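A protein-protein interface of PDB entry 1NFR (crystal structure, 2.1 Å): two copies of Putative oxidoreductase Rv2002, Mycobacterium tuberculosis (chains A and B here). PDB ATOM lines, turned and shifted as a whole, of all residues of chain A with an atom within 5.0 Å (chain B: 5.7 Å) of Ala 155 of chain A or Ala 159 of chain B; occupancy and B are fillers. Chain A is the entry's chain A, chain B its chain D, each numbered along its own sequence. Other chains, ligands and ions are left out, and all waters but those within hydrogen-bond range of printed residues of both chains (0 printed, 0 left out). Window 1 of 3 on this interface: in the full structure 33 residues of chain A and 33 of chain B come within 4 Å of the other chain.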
ATOM      1  N   TRP A 105       0.997  28.518 -26.467  1.00  0.00           N
ATOM      2  CA  TRP A 105       2.003  28.741 -25.430  1.00  0.00           C
ATOM      3  C   TRP A 105       1.322  28.788 -24.074  1.00  0.00           C
ATOM      4  O   TRP A 105       1.728  28.094 -23.140  1.00  0.00           O
ATOM      5  CB  TRP A 105       2.755  30.049 -25.708  1.00  0.00           C
ATOM      6  CG  TRP A 105       3.588  30.572 -24.572  1.00  0.00           C
ATOM      7  CD1 TRP A 105       3.200  31.461 -23.617  1.00  0.00           C
ATOM      8  CD2 TRP A 105       4.962  30.267 -24.300  1.00  0.00           C
ATOM      9  NE1 TRP A 105       4.246  31.738 -22.769  1.00  0.00           N
ATOM     10  CE2 TRP A 105       5.340  31.018 -23.166  1.00  0.00           C
ATOM     11  CE3 TRP A 105       5.911  29.435 -24.907  1.00  0.00           C
ATOM     12  CZ2 TRP A 105       6.630  30.961 -22.623  1.00  0.00           C
ATOM     13  CZ3 TRP A 105       7.197  29.379 -24.366  1.00  0.00           C
ATOM     14  CH2 TRP A 105       7.541  30.140 -23.235  1.00  0.00           C
ATOM     15  N   CYS A 150      10.100  23.902 -30.494  1.00  0.00           N
ATOM     16  CA  CYS A 150       9.513  23.154 -29.380  1.00  0.00           C
ATOM     17  C   CYS A 150       9.650  23.973 -28.096  1.00  0.00           C
ATOM     18  O   CYS A 150       9.936  23.437 -27.023  1.00  0.00           O
ATOM     19  CB  CYS A 150      10.267  21.830 -29.248  1.00  0.00           C
ATOM     20  SG  CYS A 150       9.467  20.551 -28.295  1.00  0.00           S
ATOM     21  N   HIS A 151       9.422  25.273 -28.222  1.00  0.00           N
ATOM     22  CA  HIS A 151       9.563  26.221 -27.120  1.00  0.00           C
ATOM     23  C   HIS A 151       8.617  26.047 -25.936  1.00  0.00           C
ATOM     24  O   HIS A 151       9.048  26.084 -24.780  1.00  0.00           O
ATOM     25  CB  HIS A 151       9.467  27.631 -27.702  1.00  0.00           C
ATOM     26  CG  HIS A 151      10.320  27.814 -28.915  1.00  0.00           C
ATOM     27  ND1 HIS A 151      11.693  27.679 -28.877  1.00  0.00           N
ATOM     28  CD2 HIS A 151       9.995  28.001 -30.216  1.00  0.00           C
ATOM     29  CE1 HIS A 151      12.173  27.766 -30.105  1.00  0.00           C
ATOM     30  NE2 HIS A 151      11.164  27.960 -30.937  1.00  0.00           N
ATOM     31  N   GLY A 152       7.333  25.858 -26.215  1.00  0.00           N
ATOM     32  CA  GLY A 152       6.383  25.669 -25.133  1.00  0.00           C
ATOM     33  C   GLY A 152       6.651  24.391 -24.353  1.00  0.00           C
ATOM     34  O   GLY A 152       6.727  24.404 -23.121  1.00  0.00           O
ATOM     35  N   TYR A 153       6.803  23.284 -25.073  1.00  0.00           N
ATOM     36  CA  TYR A 153       7.051  21.990 -24.446  1.00  0.00           C
ATOM     37  C   TYR A 153       8.362  22.006 -23.665  1.00  0.00           C
ATOM     38  O   TYR A 153       8.408  21.581 -22.508  1.00  0.00           O
ATOM     39  CB  TYR A 153       7.103  20.894 -25.508  1.00  0.00           C
ATOM     40  CG  TYR A 153       7.025  19.484 -24.961  1.00  0.00           C
ATOM     41  CD1 TYR A 153       5.827  18.972 -24.454  1.00  0.00           C
ATOM     42  CD2 TYR A 153       8.142  18.648 -24.981  1.00  0.00           C
ATOM     43  CE1 TYR A 153       5.742  17.656 -23.985  1.00  0.00           C
ATOM     44  CE2 TYR A 153       8.068  17.331 -24.518  1.00  0.00           C
ATOM     45  CZ  TYR A 153       6.869  16.840 -24.025  1.00  0.00           C
ATOM     46  OH  TYR A 153       6.798  15.531 -23.602  1.00  0.00           O
ATOM     47  N   THR A 154       9.424  22.492 -24.300  1.00  0.00           N
ATOM     48  CA  THR A 154      10.733  22.572 -23.656  1.00  0.00           C
ATOM     49  C   THR A 154      10.684  23.396 -22.360  1.00  0.00           C
ATOM     50  O   THR A 154      11.131  22.945 -21.305  1.00  0.00           O
ATOM     51  CB  THR A 154      11.785  23.195 -24.615  1.00  0.00           C
ATOM     52  OG1 THR A 154      12.053  22.279 -25.687  1.00  0.00           O
ATOM     53  CG2 THR A 154      13.089  23.488 -23.878  1.00  0.00           C
ATOM     54  N   ALA A 155      10.140  24.601 -22.441  1.00  0.00           N
ATOM     55  CA  ALA A 155      10.050  25.465 -21.268  1.00  0.00           C
ATOM     56  C   ALA A 155       9.262  24.809 -20.131  1.00  0.00           C
ATOM     57  O   ALA A 155       9.702  24.823 -18.982  1.00  0.00           O
ATOM     58  CB  ALA A 155       9.410  26.807 -21.648  1.00  0.00           C
ATOM     59  N   THR A 156       8.103  24.241 -20.443  1.00  0.00           N
ATOM     60  CA  THR A 156       7.296  23.602 -19.412  1.00  0.00           C
ATOM     61  C   THR A 156       7.990  22.381 -18.817  1.00  0.00           C
ATOM     62  O   THR A 156       7.928  22.163 -17.611  1.00  0.00           O
ATOM     63  CB  THR A 156       5.901  23.171 -19.944  1.00  0.00           C
ATOM     64  OG1 THR A 156       6.055  22.293 -21.065  1.00  0.00           O
ATOM     65  CG2 THR A 156       5.082  24.397 -20.351  1.00  0.00           C
ATOM     66  N   LYS A 157       8.647  21.588 -19.656  1.00  0.00           N
ATOM     67  CA  LYS A 157       9.333  20.401 -19.159  1.00  0.00           C
ATOM     68  C   LYS A 157      10.538  20.768 -18.293  1.00  0.00           C
ATOM     69  O   LYS A 157      10.903  20.016 -17.393  1.00  0.00           O
ATOM     70  CB  LYS A 157       9.739  19.486 -20.322  1.00  0.00           C
ATOM     71  CG  LYS A 157       8.543  18.786 -20.971  1.00  0.00           C
ATOM     72  CD  LYS A 157       7.746  18.007 -19.926  1.00  0.00           C
ATOM     73  CE  LYS A 157       6.532  17.320 -20.517  1.00  0.00           C
ATOM     74  NZ  LYS A 157       5.713  16.609 -19.488  1.00  0.00           N
ATOM     75  N   PHE A 158      11.153  21.919 -18.563  1.00  0.00           N
ATOM     76  CA  PHE A 158      12.277  22.382 -17.750  1.00  0.00           C
ATOM     77  C   PHE A 158      11.675  22.903 -16.440  1.00  0.00           C
ATOM     78  O   PHE A 158      12.238  22.721 -15.364  1.00  0.00           O
ATOM     79  CB  PHE A 158      13.034  23.521 -18.444  1.00  0.00           C
ATOM     80  CG  PHE A 158      14.318  23.092 -19.111  1.00  0.00           C
ATOM     81  CD1 PHE A 158      14.297  22.430 -20.332  1.00  0.00           C
ATOM     82  CD2 PHE A 158      15.547  23.347 -18.505  1.00  0.00           C
ATOM     83  CE1 PHE A 158      15.487  22.024 -20.947  1.00  0.00           C
ATOM     84  CE2 PHE A 158      16.736  22.947 -19.105  1.00  0.00           C
ATOM     85  CZ  PHE A 158      16.710  22.281 -20.330  1.00  0.00           C
ATOM     86  N   ALA A 159      10.513  23.544 -16.543  1.00  0.00           N
ATOM     87  CA  ALA A 159       9.829  24.097 -15.374  1.00  0.00           C
ATOM     88  C   ALA A 159       9.448  23.009 -14.372  1.00  0.00           C
ATOM     89  O   ALA A 159       9.569  23.199 -13.163  1.00  0.00           O
ATOM     90  CB  ALA A 159       8.585  24.869 -15.812  1.00  0.00           C
ATOM     91  N   LEU B 113       8.519  34.221 -17.331  1.00  0.00           N
ATOM     92  CA  LEU B 113       8.661  33.281 -18.435  1.00  0.00           C
ATOM     93  C   LEU B 113       8.074  33.796 -19.751  1.00  0.00           C
ATOM     94  O   LEU B 113       8.787  33.932 -20.744  1.00  0.00           O
ATOM     95  CB  LEU B 113       8.025  31.935 -18.059  1.00  0.00           C
ATOM     96  CG  LEU B 113       7.915  30.855 -19.144  1.00  0.00           C
ATOM     97  CD1 LEU B 113       9.267  30.609 -19.787  1.00  0.00           C
ATOM     98  CD2 LEU B 113       7.373  29.579 -18.523  1.00  0.00           C
ATOM     99  N   THR B 154      11.439  29.517  -8.997  1.00  0.00           N
ATOM    100  CA  THR B 154      12.245  28.381  -9.431  1.00  0.00           C
ATOM    101  C   THR B 154      11.771  27.836 -10.779  1.00  0.00           C
ATOM    102  O   THR B 154      12.566  27.633 -11.697  1.00  0.00           O
ATOM    103  CB  THR B 154      12.190  27.248  -8.388  1.00  0.00           C
ATOM    104  OG1 THR B 154      12.837  27.680  -7.189  1.00  0.00           O
ATOM    105  CG2 THR B 154      12.882  25.998  -8.911  1.00  0.00           C
ATOM    106  N   ALA B 155      10.467  27.609 -10.886  1.00  0.00           N
ATOM    107  CA  ALA B 155       9.867  27.100 -12.109  1.00  0.00           C
ATOM    108  C   ALA B 155      10.161  27.989 -13.314  1.00  0.00           C
ATOM    109  O   ALA B 155      10.628  27.510 -14.347  1.00  0.00           O
ATOM    110  CB  ALA B 155       8.364  26.964 -11.921  1.00  0.00           C
ATOM    111  N   THR B 156       9.893  29.285 -13.182  1.00  0.00           N
ATOM    112  CA  THR B 156      10.126  30.212 -14.283  1.00  0.00           C
ATOM    113  C   THR B 156      11.604  30.339 -14.653  1.00  0.00           C
ATOM    114  O   THR B 156      11.944  30.409 -15.837  1.00  0.00           O
ATOM    115  CB  THR B 156       9.542  31.622 -13.979  1.00  0.00           C
ATOM    116  OG1 THR B 156      10.105  32.137 -12.767  1.00  0.00           O
ATOM    117  CG2 THR B 156       8.021  31.543 -13.836  1.00  0.00           C
ATOM    118  N   LYS B 157      12.480  30.370 -13.654  1.00  0.00           N
ATOM    119  CA  LYS B 157      13.909  30.478 -13.932  1.00  0.00           C
ATOM    120  C   LYS B 157      14.432  29.212 -14.614  1.00  0.00           C
ATOM    121  O   LYS B 157      15.367  29.273 -15.409  1.00  0.00           O
ATOM    122  CB  LYS B 157      14.685  30.777 -12.642  1.00  0.00           C
ATOM    123  CG  LYS B 157      14.397  32.180 -12.099  1.00  0.00           C
ATOM    124  CD  LYS B 157      14.594  33.249 -13.199  1.00  0.00           C
ATOM    125  CE  LYS B 157      14.462  34.686 -12.664  1.00  0.00           C
ATOM    126  NZ  LYS B 157      14.755  35.724 -13.725  1.00  0.00           N
ATOM    127  N   PHE B 158      13.829  28.064 -14.303  1.00  0.00           N
ATOM    128  CA  PHE B 158      14.219  26.819 -14.953  1.00  0.00           C
ATOM    129  C   PHE B 158      13.670  26.894 -16.373  1.00  0.00           C
ATOM    130  O   PHE B 158      14.326  26.486 -17.325  1.00  0.00           O
ATOM    131  CB  PHE B 158      13.610  25.606 -14.245  1.00  0.00           C
ATOM    132  CG  PHE B 158      14.553  24.908 -13.316  1.00  0.00           C
ATOM    133  CD1 PHE B 158      14.850  25.445 -12.069  1.00  0.00           C
ATOM    134  CD2 PHE B 158      15.169  23.721 -13.700  1.00  0.00           C
ATOM    135  CE1 PHE B 158      15.751  24.806 -11.212  1.00  0.00           C
ATOM    136  CE2 PHE B 158      16.070  23.077 -12.855  1.00  0.00           C
ATOM    137  CZ  PHE B 158      16.363  23.619 -11.609  1.00  0.00           C
ATOM    138  N   ALA B 159      12.455  27.430 -16.498  1.00  0.00           N
ATOM    139  CA  ALA B 159      11.801  27.570 -17.797  1.00  0.00           C
ATOM    140  C   ALA B 159      12.636  28.441 -18.726  1.00  0.00           C
ATOM    141  O   ALA B 159      12.833  28.100 -19.896  1.00  0.00           O
ATOM    142  CB  ALA B 159      10.406  28.177 -17.626  1.00  0.00           C
ATOM    143  N   VAL B 160      13.115  29.569 -18.203  1.00  0.00           N
ATOM    144  CA  VAL B 160      13.937  30.492 -18.983  1.00  0.00           C
ATOM    145  C   VAL B 160      15.220  29.802 -19.433  1.00  0.00           C
ATOM    146  O   VAL B 160      15.723  30.047 -20.536  1.00  0.00           O
ATOM    147  CB  VAL B 160      14.284  31.751 -18.160  1.00  0.00           C
ATOM    148  CG1 VAL B 160      15.386  32.566 -18.861  1.00  0.00           C
ATOM    149  CG2 VAL B 160      13.025  32.601 -17.987  1.00  0.00           C
ATOM    150  N   ARG B 161      15.738  28.936 -18.567  1.00  0.00           N
ATOM    151  CA  ARG B 161      16.949  28.173 -18.850  1.00  0.00           C
ATOM    152  C   ARG B 161      16.698  27.259 -20.055  1.00  0.00           C
ATOM    153  O   ARG B 161      17.526  27.164 -20.958  1.00  0.00           O
ATOM    154  CB  ARG B 161      17.318  27.341 -17.618  1.00  0.00           C
ATOM    155  CG  ARG B 161      18.540  26.453 -17.765  1.00  0.00           C
ATOM    156  CD  ARG B 161      18.687  25.597 -16.523  1.00  0.00           C
ATOM    157  NE  ARG B 161      19.731  24.585 -16.638  1.00  0.00           N
ATOM    158  CZ  ARG B 161      19.890  23.587 -15.776  1.00  0.00           C
ATOM    159  NH1 ARG B 161      19.075  23.464 -14.736  1.00  0.00           N
ATOM    160  NH2 ARG B 161      20.863  22.708 -15.957  1.00  0.00           N
ATOM    161  N   GLY B 162      15.543  26.594 -20.062  1.00  0.00           N
ATOM    162  CA  GLY B 162      15.201  25.705 -21.162  1.00  0.00           C
ATOM    163  C   GLY B 162      14.840  26.435 -22.451  1.00  0.00           C
ATOM    164  O   GLY B 162      15.241  26.023 -23.545  1.00  0.00           O
ATOM    165  N   LEU B 163      14.064  27.509 -22.325  1.00  0.00           N
ATOM    166  CA  LEU B 163      13.655  28.299 -23.487  1.00  0.00           C
ATOM    167  C   LEU B 163      14.890  28.823 -24.210  1.00  0.00           C
ATOM    168  O   LEU B 163      14.907  28.953 -25.437  1.00  0.00           O
ATOM    169  CB  LEU B 163      12.788  29.484 -23.044  1.00  0.00           C
ATOM    170  CG  LEU B 163      12.334  30.448 -24.152  1.00  0.00           C
ATOM    171  CD1 LEU B 163      11.402  29.729 -25.141  1.00  0.00           C
ATOM    172  CD2 LEU B 163      11.635  31.637 -23.517  1.00  0.00           C
ATOM    173  N   THR B 164      15.924  29.127 -23.439  1.00  0.00           N
ATOM    174  CA  THR B 164      17.167  29.631 -24.001  1.00  0.00           C
ATOM    175  C   THR B 164      17.758  28.638 -24.997  1.00  0.00           C
ATOM    176  O   THR B 164      18.231  29.019 -26.064  1.00  0.00           O
ATOM    177  CB  THR B 164      18.215  29.880 -22.897  1.00  0.00           C
ATOM    178  OG1 THR B 164      17.772  30.948 -22.050  1.00  0.00           O
ATOM    179  CG2 THR B 164      19.571  30.234 -23.511  1.00  0.00           C
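The backbone carbonyl oxygen (O) of Cys 150 of chain A is in hydrogen-bond range of the side-chain hydroxyl (OG1) of Thr 154 of chain A (2.8 Å).
Leu 113 of chain B touches Trp 105 of chain A. Leu 163 of chain B touches His 151 of chain A. Thr 154 of chain A touches Gly 162 of chain B (CG2 to O, 3.3 Å). Ala 159 of chain B touches Ala 155 of chain A (CA to O, 3.7 Å). Phe 158 of chain B touches Phe 158 of chain A (CB to O, 3.4 Å). CG of Phe 158 of chain A touches CA of Gly 162 of chain B (3.4 Å). Ala 155 of chain B touches Ala 159 of chain A.
Of the printed residues of chain B, Thr 154 of chain A touches Gly 162. Ala 155 of chain A touches just one residue of chain B: Ala 159. Of the printed residues of chain B, Ala 159 of chain A touches Ala 155. Of the printed residues of chain A, Leu 113 of chain B touches Trp 105. Lys 157 of chain B touches none of the printed residues of chain A. Of the printed residues of chain A, Phe 158 of chain B touches Phe 158. Ala 159 of chain B touches just one residue of chain A: Ala 155. Of the printed residues of chain A, Gly 162 of chain B touches Thr 154 (3.3 Å) and Phe 158 (3.4 Å). The nearest residue of chain B that does not touch Ala 155 of chain A is Leu 113 of chain B (4.2 Å). The nearest printed residue of chain A that does not touch Leu 163 of chain B is Trp 105 of chain A (4.3 Å).
Of the 11 printed residues of chain A, 6 touch a printed residue of chain B. Hydrophobic or aromatic side chains of chain A within 4 Å of the printed part of chain B: Trp 105, His 151, Phe 158 and Ala 159. Of the 12 printed residues of chain B, 6 touch a printed residue of chain A. Printed residues of chain B that touch a printed residue of chain A: Leu 113, Ala 155, Phe 158, Ala 159, Gly 162 and Leu 163. Among the printed residues, 7 pairs touch across the chains. Among the printed residues, no Asp or Glu carboxylate lies within 4 Å of a Lys or Arg side-chain nitrogen of the other chain.
Ala 155 of chain A touches Ala 159 of chain B, and with the chains exchanged Ala 159 of chain A touches Ala 155 of chain B. Phe 158 of chain B touches its own counterpart, Phe 158 of chain A. 6 positions are printed for both chains. Of the 7 pairs that touch across the chains among the printed residues, 3 have their exchanged pair printed and touching as well.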
